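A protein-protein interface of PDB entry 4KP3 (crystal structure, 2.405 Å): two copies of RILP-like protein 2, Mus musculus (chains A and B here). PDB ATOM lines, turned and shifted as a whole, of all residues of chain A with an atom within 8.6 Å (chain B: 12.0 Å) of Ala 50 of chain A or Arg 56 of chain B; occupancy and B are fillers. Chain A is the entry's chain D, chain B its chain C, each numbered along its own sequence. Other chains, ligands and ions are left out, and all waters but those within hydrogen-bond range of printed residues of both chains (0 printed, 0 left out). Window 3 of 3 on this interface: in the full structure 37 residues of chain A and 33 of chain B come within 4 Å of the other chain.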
ATOM      1  N   VAL A  43       0.038 -12.081 -20.891  1.00  0.00           N
ATOM      2  CA  VAL A  43      -0.655 -10.797 -20.861  1.00  0.00           C
ATOM      3  C   VAL A  43      -0.970 -10.334 -19.435  1.00  0.00           C
ATOM      4  O   VAL A  43      -0.969  -9.136 -19.158  1.00  0.00           O
ATOM      5  CB  VAL A  43      -1.898 -10.759 -21.784  1.00  0.00           C
ATOM      6  CG1 VAL A  43      -1.933 -11.980 -22.684  1.00  0.00           C
ATOM      7  CG2 VAL A  43      -3.169 -10.629 -20.979  1.00  0.00           C
ATOM      8  N   VAL A  44      -1.211 -11.278 -18.530  1.00  0.00           N
ATOM      9  CA  VAL A  44      -1.369 -10.930 -17.123  1.00  0.00           C
ATOM     10  C   VAL A  44      -0.035 -10.412 -16.586  1.00  0.00           C
ATOM     11  O   VAL A  44       0.005  -9.442 -15.826  1.00  0.00           O
ATOM     12  CB  VAL A  44      -1.893 -12.128 -16.287  1.00  0.00           C
ATOM     13  CG1 VAL A  44      -1.641 -11.914 -14.806  1.00  0.00           C
ATOM     14  CG2 VAL A  44      -3.374 -12.351 -16.548  1.00  0.00           C
ATOM     15  N   GLY A  45       1.055 -11.050 -17.007  1.00  0.00           N
ATOM     16  CA  GLY A  45       2.395 -10.595 -16.669  1.00  0.00           C
ATOM     17  C   GLY A  45       2.673  -9.160 -17.090  1.00  0.00           C
ATOM     18  O   GLY A  45       3.228  -8.380 -16.317  1.00  0.00           O
ATOM     19  N   ARG A  46       2.281  -8.810 -18.314  1.00  0.00           N
ATOM     20  CA  ARG A  46       2.461  -7.450 -18.821  1.00  0.00           C
ATOM     21  C   ARG A  46       1.713  -6.439 -17.971  1.00  0.00           C
ATOM     22  O   ARG A  46       2.239  -5.381 -17.622  1.00  0.00           O
ATOM     23  CB  ARG A  46       1.965  -7.333 -20.267  1.00  0.00           C
ATOM     24  CG  ARG A  46       2.837  -8.000 -21.307  1.00  0.00           C
ATOM     25  CD  ARG A  46       2.483  -7.497 -22.702  1.00  0.00           C
ATOM     26  NE  ARG A  46       1.038  -7.436 -22.923  1.00  0.00           N
ATOM     27  CZ  ARG A  46       0.436  -7.776 -24.059  1.00  0.00           C
ATOM     28  NH1 ARG A  46       1.152  -8.211 -25.089  1.00  0.00           N
ATOM     29  NH2 ARG A  46      -0.882  -7.685 -24.166  1.00  0.00           N
ATOM     30  N   GLU A  47       0.469  -6.763 -17.649  1.00  0.00           N
ATOM     31  CA  GLU A  47      -0.364  -5.844 -16.893  1.00  0.00           C
ATOM     32  C   GLU A  47       0.153  -5.669 -15.470  1.00  0.00           C
ATOM     33  O   GLU A  47       0.133  -4.563 -14.932  1.00  0.00           O
ATOM     34  CB  GLU A  47      -1.819  -6.291 -16.939  1.00  0.00           C
ATOM     35  CG  GLU A  47      -2.364  -6.245 -18.355  1.00  0.00           C
ATOM     36  CD  GLU A  47      -3.832  -6.587 -18.442  1.00  0.00           C
ATOM     37  OE1 GLU A  47      -4.533  -6.492 -17.414  1.00  0.00           O
ATOM     38  OE2 GLU A  47      -4.286  -6.948 -19.548  1.00  0.00           O
ATOM     39  N   LEU A  48       0.645  -6.754 -14.879  1.00  0.00           N
ATOM     40  CA  LEU A  48       1.281  -6.678 -13.565  1.00  0.00           C
ATOM     41  C   LEU A  48       2.554  -5.837 -13.618  1.00  0.00           C
ATOM     42  O   LEU A  48       2.785  -4.996 -12.751  1.00  0.00           O
ATOM     43  CB  LEU A  48       1.600  -8.077 -13.033  1.00  0.00           C
ATOM     44  CG  LEU A  48       0.436  -8.865 -12.434  1.00  0.00           C
ATOM     45  CD1 LEU A  48       0.770 -10.344 -12.381  1.00  0.00           C
ATOM     46  CD2 LEU A  48       0.102  -8.339 -11.044  1.00  0.00           C
ATOM     47  N   MET A  49       3.372  -6.073 -14.641  1.00  0.00           N
ATOM     48  CA  MET A  49       4.620  -5.336 -14.824  1.00  0.00           C
ATOM     49  C   MET A  49       4.374  -3.842 -15.013  1.00  0.00           C
ATOM     50  O   MET A  49       5.105  -3.011 -14.479  1.00  0.00           O
ATOM     51  CB  MET A  49       5.404  -5.902 -16.017  1.00  0.00           C
ATOM     52  CG  MET A  49       6.696  -5.158 -16.337  1.00  0.00           C
ATOM     53  SD  MET A  49       7.607  -5.894 -17.710  1.00  0.00           S
ATOM     54  CE  MET A  49       6.470  -5.632 -19.071  1.00  0.00           C
ATOM     55  N   ALA A  50       3.330  -3.505 -15.763  1.00  0.00           N
ATOM     56  CA  ALA A  50       2.983  -2.108 -15.991  1.00  0.00           C
ATOM     57  C   ALA A  50       2.494  -1.395 -14.722  1.00  0.00           C
ATOM     58  O   ALA A  50       2.262  -0.188 -14.740  1.00  0.00           O
ATOM     59  CB  ALA A  50       1.954  -1.991 -17.102  1.00  0.00           C
ATOM     60  N   LEU A  51       2.326  -2.134 -13.627  1.00  0.00           N
ATOM     61  CA  LEU A  51       1.880  -1.523 -12.372  1.00  0.00           C
ATOM     62  C   LEU A  51       3.033  -1.088 -11.475  1.00  0.00           C
ATOM     63  O   LEU A  51       2.815  -0.463 -10.435  1.00  0.00           O
ATOM     64  CB  LEU A  51       0.951  -2.453 -11.599  1.00  0.00           C
ATOM     65  CG  LEU A  51      -0.426  -2.682 -12.208  1.00  0.00           C
ATOM     66  CD1 LEU A  51      -1.231  -3.583 -11.297  1.00  0.00           C
ATOM     67  CD2 LEU A  51      -1.134  -1.360 -12.436  1.00  0.00           C
ATOM     68  N   GLY A  52       4.255  -1.431 -11.868  1.00  0.00           N
ATOM     69  CA  GLY A  52       5.430  -0.920 -11.186  1.00  0.00           C
ATOM     70  C   GLY A  52       6.046  -1.833 -10.149  1.00  0.00           C
ATOM     71  O   GLY A  52       5.744  -3.025 -10.088  1.00  0.00           O
ATOM     72  N   SER A  53       6.911  -1.254  -9.321  1.00  0.00           N
ATOM     73  CA  SER A  53       7.734  -2.022  -8.391  1.00  0.00           C
ATOM     74  C   SER A  53       7.227  -2.013  -6.950  1.00  0.00           C
ATOM     75  O   SER A  53       7.969  -2.364  -6.032  1.00  0.00           O
ATOM     76  CB  SER A  53       9.182  -1.524  -8.429  1.00  0.00           C
ATOM     77  OG  SER A  53       9.760  -1.742  -9.705  1.00  0.00           O
ATOM     78  N   VAL A  57       2.548  -5.227  -5.175  1.00  0.00           N
ATOM     79  CA  VAL A  57       2.253  -5.646  -6.540  1.00  0.00           C
ATOM     80  C   VAL A  57       3.018  -6.939  -6.819  1.00  0.00           C
ATOM     81  O   VAL A  57       2.489  -7.868  -7.431  1.00  0.00           O
ATOM     82  CB  VAL A  57       2.613  -4.558  -7.577  1.00  0.00           C
ATOM     83  CG1 VAL A  57       2.664  -5.137  -8.988  1.00  0.00           C
ATOM     84  CG2 VAL A  57       1.612  -3.416  -7.510  1.00  0.00           C
ATOM     85  N   GLN A  61       1.826 -10.582  -7.698  1.00  0.00           N
ATOM     86  CA  GLN A  61       2.362 -11.206  -8.905  1.00  0.00           C
ATOM     87  C   GLN A  61       2.690 -12.683  -8.689  1.00  0.00           C
ATOM     88  O   GLN A  61       2.235 -13.549  -9.439  1.00  0.00           O
ATOM     89  CB  GLN A  61       3.605 -10.451  -9.382  1.00  0.00           C
ATOM     90  CG  GLN A  61       4.196 -10.936 -10.697  1.00  0.00           C
ATOM     91  CD  GLN A  61       5.516 -10.248 -11.010  1.00  0.00           C
ATOM     92  OE1 GLN A  61       6.379 -10.124 -10.142  1.00  0.00           O
ATOM     93  NE2 GLN A  61       5.670  -9.781 -12.247  1.00  0.00           N
ATOM     94  N   VAL B  44      -7.057 -12.667  -2.812  1.00  0.00           N
ATOM     95  CA  VAL B  44      -6.549 -11.941  -3.968  1.00  0.00           C
ATOM     96  C   VAL B  44      -7.426 -10.719  -4.221  1.00  0.00           C
ATOM     97  O   VAL B  44      -6.933  -9.653  -4.599  1.00  0.00           O
ATOM     98  CB  VAL B  44      -6.489 -12.842  -5.222  1.00  0.00           C
ATOM     99  CG1 VAL B  44      -6.407 -12.011  -6.488  1.00  0.00           C
ATOM    100  CG2 VAL B  44      -5.309 -13.806  -5.129  1.00  0.00           C
ATOM    101  N   GLU B  47      -6.283  -7.944  -1.963  1.00  0.00           N
ATOM    102  CA  GLU B  47      -4.982  -7.439  -2.384  1.00  0.00           C
ATOM    103  C   GLU B  47      -5.088  -6.530  -3.599  1.00  0.00           C
ATOM    104  O   GLU B  47      -4.347  -5.554  -3.721  1.00  0.00           O
ATOM    105  CB  GLU B  47      -4.026  -8.598  -2.660  1.00  0.00           C
ATOM    106  CG  GLU B  47      -3.615  -9.326  -1.399  1.00  0.00           C
ATOM    107  CD  GLU B  47      -2.565 -10.386  -1.645  1.00  0.00           C
ATOM    108  OE1 GLU B  47      -1.697 -10.189  -2.531  1.00  0.00           O
ATOM    109  OE2 GLU B  47      -2.610 -11.416  -0.943  1.00  0.00           O
ATOM    110  N   LEU B  48      -6.010  -6.863  -4.495  1.00  0.00           N
ATOM    111  CA  LEU B  48      -6.302  -6.020  -5.642  1.00  0.00           C
ATOM    112  C   LEU B  48      -6.996  -4.746  -5.181  1.00  0.00           C
ATOM    113  O   LEU B  48      -6.707  -3.654  -5.672  1.00  0.00           O
ATOM    114  CB  LEU B  48      -7.198  -6.765  -6.629  1.00  0.00           C
ATOM    115  CG  LEU B  48      -6.513  -7.796  -7.519  1.00  0.00           C
ATOM    116  CD1 LEU B  48      -7.538  -8.776  -8.067  1.00  0.00           C
ATOM    117  CD2 LEU B  48      -5.762  -7.089  -8.653  1.00  0.00           C
ATOM    118  N   MET B  49      -7.913  -4.900  -4.232  1.00  0.00           N
ATOM    119  CA  MET B  49      -8.635  -3.767  -3.667  1.00  0.00           C
ATOM    120  C   MET B  49      -7.670  -2.762  -3.044  1.00  0.00           C
ATOM    121  O   MET B  49      -7.844  -1.555  -3.185  1.00  0.00           O
ATOM    122  CB  MET B  49      -9.654  -4.239  -2.623  1.00  0.00           C
ATOM    123  CG  MET B  49     -11.108  -3.970  -2.994  1.00  0.00           C
ATOM    124  SD  MET B  49     -12.024  -5.456  -3.468  1.00  0.00           S
ATOM    125  CE  MET B  49     -13.518  -4.729  -4.142  1.00  0.00           C
ATOM    126  N   ALA B  50      -6.640  -3.266  -2.371  1.00  0.00           N
ATOM    127  CA  ALA B  50      -5.690  -2.406  -1.665  1.00  0.00           C
ATOM    128  C   ALA B  50      -4.845  -1.516  -2.582  1.00  0.00           C
ATOM    129  O   ALA B  50      -4.268  -0.527  -2.128  1.00  0.00           O
ATOM    130  CB  ALA B  50      -4.793  -3.241  -0.755  1.00  0.00           C
ATOM    131  N   LEU B  51      -4.769  -1.866  -3.863  1.00  0.00           N
ATOM    132  CA  LEU B  51      -3.926  -1.126  -4.798  1.00  0.00           C
ATOM    133  C   LEU B  51      -4.598   0.145  -5.293  1.00  0.00           C
ATOM    134  O   LEU B  51      -3.939   1.027  -5.839  1.00  0.00           O
ATOM    135  CB  LEU B  51      -3.543  -1.997  -5.994  1.00  0.00           C
ATOM    136  CG  LEU B  51      -2.768  -3.275  -5.697  1.00  0.00           C
ATOM    137  CD1 LEU B  51      -2.493  -4.000  -6.994  1.00  0.00           C
ATOM    138  CD2 LEU B  51      -1.476  -2.965  -4.962  1.00  0.00           C
ATOM    139  N   GLY B  52      -5.912   0.229  -5.117  1.00  0.00           N
ATOM    140  CA  GLY B  52      -6.646   1.418  -5.502  1.00  0.00           C
ATOM    141  C   GLY B  52      -7.597   1.210  -6.664  1.00  0.00           C
ATOM    142  O   GLY B  52      -7.900   0.080  -7.042  1.00  0.00           O
ATOM    143  N   SER B  53      -8.057   2.316  -7.240  1.00  0.00           N
ATOM    144  CA  SER B  53      -9.082   2.280  -8.275  1.00  0.00           C
ATOM    145  C   SER B  53      -8.554   2.648  -9.662  1.00  0.00           C
ATOM    146  O   SER B  53      -9.321   3.064 -10.532  1.00  0.00           O
ATOM    147  CB  SER B  53     -10.240   3.206  -7.891  1.00  0.00           C
ATOM    148  OG  SER B  53     -10.727   2.896  -6.595  1.00  0.00           O
ATOM    149  N   ASP B  54      -7.246   2.507  -9.855  1.00  0.00           N
ATOM    150  CA  ASP B  54      -6.631   2.635 -11.173  1.00  0.00           C
ATOM    151  C   ASP B  54      -7.365   1.714 -12.147  1.00  0.00           C
ATOM    152  O   ASP B  54      -7.536   0.530 -11.868  1.00  0.00           O
ATOM    153  CB  ASP B  54      -5.150   2.241 -11.082  1.00  0.00           C
ATOM    154  CG  ASP B  54      -4.359   2.579 -12.341  1.00  0.00           C
ATOM    155  OD1 ASP B  54      -4.923   2.539 -13.453  1.00  0.00           O
ATOM    156  OD2 ASP B  54      -3.152   2.878 -12.215  1.00  0.00           O
ATOM    157  N   PRO B  55      -7.818   2.261 -13.287  1.00  0.00           N
ATOM    158  CA  PRO B  55      -8.502   1.459 -14.310  1.00  0.00           C
ATOM    159  C   PRO B  55      -7.713   0.234 -14.776  1.00  0.00           C
ATOM    160  O   PRO B  55      -8.324  -0.755 -15.180  1.00  0.00           O
ATOM    161  CB  PRO B  55      -8.682   2.445 -15.476  1.00  0.00           C
ATOM    162  CG  PRO B  55      -7.831   3.639 -15.139  1.00  0.00           C
ATOM    163  CD  PRO B  55      -7.782   3.687 -13.648  1.00  0.00           C
ATOM    164  N   ARG B  56      -6.387   0.284 -14.730  1.00  0.00           N
ATOM    165  CA  ARG B  56      -5.619  -0.871 -15.176  1.00  0.00           C
ATOM    166  C   ARG B  56      -5.430  -1.892 -14.058  1.00  0.00           C
ATOM    167  O   ARG B  56      -5.174  -3.067 -14.319  1.00  0.00           O
ATOM    168  CB  ARG B  56      -4.299  -0.469 -15.852  1.00  0.00           C
ATOM    169  CG  ARG B  56      -3.354   0.338 -15.004  1.00  0.00           C
ATOM    170  CD  ARG B  56      -2.299   1.019 -15.859  1.00  0.00           C
ATOM    171  NE  ARG B  56      -1.397   1.807 -15.028  1.00  0.00           N
ATOM    172  CZ  ARG B  56      -0.115   2.019 -15.303  1.00  0.00           C
ATOM    173  NH1 ARG B  56       0.426   1.506 -16.400  1.00  0.00           N
ATOM    174  NH2 ARG B  56       0.626   2.745 -14.478  1.00  0.00           N
ATOM    175  N   VAL B  57      -5.580  -1.445 -12.815  1.00  0.00           N
ATOM    176  CA  VAL B  57      -5.724  -2.371 -11.697  1.00  0.00           C
ATOM    177  C   VAL B  57      -7.065  -3.087 -11.830  1.00  0.00           C
ATOM    178  O   VAL B  57      -7.144  -4.310 -11.705  1.00  0.00           O
ATOM    179  CB  VAL B  57      -5.650  -1.651 -10.337  1.00  0.00           C
ATOM    180  CG1 VAL B  57      -6.120  -2.569  -9.218  1.00  0.00           C
ATOM    181  CG2 VAL B  57      -4.230  -1.160 -10.071  1.00  0.00           C
ATOM    182  N   THR B  58      -8.110  -2.312 -12.111  1.00  0.00           N
ATOM    183  CA  THR B  58      -9.446  -2.860 -12.306  1.00  0.00           C
ATOM    184  C   THR B  58      -9.497  -3.833 -13.489  1.00  0.00           C
ATOM    185  O   THR B  58     -10.146  -4.877 -13.404  1.00  0.00           O
ATOM    186  CB  THR B  58     -10.513  -1.744 -12.467  1.00  0.00           C
ATOM    187  OG1 THR B  58     -10.578  -0.970 -11.264  1.00  0.00           O
ATOM    188  CG2 THR B  58     -11.888  -2.334 -12.746  1.00  0.00           C
ATOM    189  N   ARG B  59      -8.803  -3.506 -14.576  1.00  0.00           N
ATOM    190  CA  ARG B  59      -8.722  -4.405 -15.729  1.00  0.00           C
ATOM    191  C   ARG B  59      -8.077  -5.729 -15.354  1.00  0.00           C
ATOM    192  O   ARG B  59      -8.552  -6.794 -15.746  1.00  0.00           O
ATOM    193  CB  ARG B  59      -7.933  -3.776 -16.875  1.00  0.00           C
ATOM    194  CG  ARG B  59      -8.730  -2.826 -17.742  1.00  0.00           C
ATOM    195  CD  ARG B  59      -8.151  -2.771 -19.147  1.00  0.00           C
ATOM    196  NE  ARG B  59      -6.691  -2.725 -19.135  1.00  0.00           N
ATOM    197  CZ  ARG B  59      -5.978  -1.610 -19.011  1.00  0.00           C
ATOM    198  NH1 ARG B  59      -6.591  -0.440 -18.886  1.00  0.00           N
ATOM    199  NH2 ARG B  59      -4.653  -1.666 -19.009  1.00  0.00           N
ATOM    200  N   LEU B  60      -6.980  -5.645 -14.611  1.00  0.00           N
ATOM    201  CA  LEU B  60      -6.288  -6.826 -14.123  1.00  0.00           C
ATOM    202  C   LEU B  60      -7.231  -7.657 -13.259  1.00  0.00           C
ATOM    203  O   LEU B  60      -7.289  -8.883 -13.369  1.00  0.00           O
ATOM    204  CB  LEU B  60      -5.058  -6.419 -13.312  1.00  0.00           C
ATOM    205  CG  LEU B  60      -4.412  -7.538 -12.494  1.00  0.00           C
ATOM    206  CD1 LEU B  60      -3.884  -8.647 -13.403  1.00  0.00           C
ATOM    207  CD2 LEU B  60      -3.306  -6.981 -11.608  1.00  0.00           C
ATOM    208  N   GLN B  61      -7.975  -6.964 -12.407  1.00  0.00           N
ATOM    209  CA  GLN B  61      -8.927  -7.592 -11.499  1.00  0.00           C
ATOM    210  C   GLN B  61      -9.949  -8.470 -12.234  1.00  0.00           C
ATOM    211  O   GLN B  61     -10.194  -9.605 -11.838  1.00  0.00           O
ATOM    212  CB  GLN B  61      -9.616  -6.506 -10.676  1.00  0.00           C
ATOM    213  CG  GLN B  61     -10.804  -6.935  -9.844  1.00  0.00           C
ATOM    214  CD  GLN B  61     -11.544  -5.735  -9.286  1.00  0.00           C
ATOM    215  OE1 GLN B  61     -12.044  -4.898 -10.039  1.00  0.00           O
ATOM    216  NE2 GLN B  61     -11.595  -5.629  -7.962  1.00  0.00           N
ATOM    217  N   PHE B  62     -10.523  -7.965 -13.319  1.00  0.00           N
ATOM    218  CA  PHE B  62     -11.496  -8.758 -14.061  1.00  0.00           C
ATOM    219  C   PHE B  62     -10.902  -9.908 -14.878  1.00  0.00           C
ATOM    220  O   PHE B  62     -11.601 -10.876 -15.179  1.00  0.00           O
ATOM    221  CB  PHE B  62     -12.415  -7.869 -14.899  1.00  0.00           C
ATOM    222  CG  PHE B  62     -13.442  -7.152 -14.075  1.00  0.00           C
ATOM    223  CD1 PHE B  62     -14.584  -7.810 -13.646  1.00  0.00           C
ATOM    224  CD2 PHE B  62     -13.245  -5.839 -13.684  1.00  0.00           C
ATOM    225  CE1 PHE B  62     -15.527  -7.162 -12.873  1.00  0.00           C
ATOM    226  CE2 PHE B  62     -14.182  -5.188 -12.904  1.00  0.00           C
ATOM    227  CZ  PHE B  62     -15.324  -5.850 -12.498  1.00  0.00           C
ATOM    228  N   LYS B  63      -9.619  -9.819 -15.220  1.00  0.00           N
ATOM    229  CA  LYS B  63      -8.951 -10.947 -15.859  1.00  0.00           C
ATOM    230  C   LYS B  63      -8.733 -12.068 -14.848  1.00  0.00           C
ATOM    231  O   LYS B  63      -8.859 -13.245 -15.173  1.00  0.00           O
ATOM    232  CB  LYS B  63      -7.629 -10.522 -16.503  1.00  0.00           C
ATOM    233  CG  LYS B  63      -7.826  -9.548 -17.646  1.00  0.00           C
ATOM    234  CD  LYS B  63      -6.712  -9.621 -18.670  1.00  0.00           C
ATOM    235  CE  LYS B  63      -7.051  -8.746 -19.868  1.00  0.00           C
ATOM    236  NZ  LYS B  63      -6.010  -8.808 -20.925  1.00  0.00           N
ATOM    237  N   ILE B  64      -8.427 -11.683 -13.615  1.00  0.00           N
ATOM    238  CA  ILE B  64      -8.265 -12.637 -12.525  1.00  0.00           C
ATOM    239  C   ILE B  64      -9.585 -13.317 -12.174  1.00  0.00           C
ATOM    240  O   ILE B  64      -9.618 -14.512 -11.875  1.00  0.00           O
ATOM    241  CB  ILE B  64      -7.671 -11.961 -11.288  1.00  0.00           C
ATOM    242  CG1 ILE B  64      -6.263 -11.457 -11.608  1.00  0.00           C
ATOM    243  CG2 ILE B  64      -7.630 -12.921 -10.106  1.00  0.00           C
ATOM    244  CD1 ILE B  64      -5.572 -10.838 -10.435  1.00  0.00           C
ATOM    245  N   VAL B  65     -10.674 -12.554 -12.227  1.00  0.00           N
ATOM    246  CA  VAL B  65     -11.998 -13.123 -12.046  1.00  0.00           C
ATOM    247  C   VAL B  65     -12.199 -14.255 -13.048  1.00  0.00           C
ATOM    248  O   VAL B  65     -12.611 -15.353 -12.675  1.00  0.00           O
ATOM    249  CB  VAL B  65     -13.115 -12.067 -12.205  1.00  0.00           C
ATOM    250  CG1 VAL B  65     -14.475 -12.737 -12.297  1.00  0.00           C
ATOM    251  CG2 VAL B  65     -13.082 -11.073 -11.055  1.00  0.00           C
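Among the printed residues, merely in contact across the chains: Val 43 of chain A with Lys 63 of chain B, Glu 47 of chain A with Leu 60 of chain B, Leu 48 of chain A with Leu 60 of chain B, Leu 51 of chain A with Arg 56 of chain B, Leu 51 of chain A with Val 57 of chain B and Leu 51 of chain A with Leu 60 of chain B.
Leu 51 of chain A touches Val 57 of chain B, but with the chains exchanged Val 57 of chain A does not touch Leu 51 of chain B (4.03 Å). 10 positions are printed for both chains. Of the 8 pairs that touch across the chains among the printed residues, none has its exchanged pair printed and touching as well.
Of the printed residues of chain B, Val 43 of chain A touches Lys 63 (3.4 Å). No residue of chain B comes within 4 Å of Met 49 of chain A. Of chain B, only Arg 56 (3.0 Å) comes within 4 Å of Ala 50 of chain A. Gly 52 of chain A touches none of the printed residues of chain B. Pro 55 of chain B touches none of the printed residues of chain A. Of the printed residues of chain A, Leu 60 of chain B touches Glu 47 (3.7 Å), Leu 48 (3.7 Å) and Leu 51 (3.99 Å). The nearest residue of chain B that does not touch Ala 50 of chain A is Asp 54 of chain B (6.7 Å). The nearest printed residue of chain A that does not touch Leu 60 of chain B is Val 44 of chain A (4.2 Å).
The guanidinium group (NH1) of Arg 56 of chain B lies within hydrogen-bond range of the backbone carbonyl oxygen (O) of Ala 50 of chain A, at 3.0 Å. NZ of Lys 63 of chain B is in salt-bridge range of OE2 of Glu 47 of chain A (2.9 Å).
The guanidinium group (NE) of Arg 56 of chain B is in salt-bridge range of the side-chain carboxylate (OD2) of Asp 54 of chain B.
Of the 13 printed residues of chain A, 5 touch a printed residue of chain B. Hydrophobic or aromatic side chains of chain A within 4 Å of the printed part of chain B: Val 43, Leu 48, Ala 50 and Leu 51. Hydrophobic or aromatic side chains of chain B within 4 Å of the printed part of chain A: Val 57 and Leu 60. Among the printed residues, 8 pairs touch across the chains.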
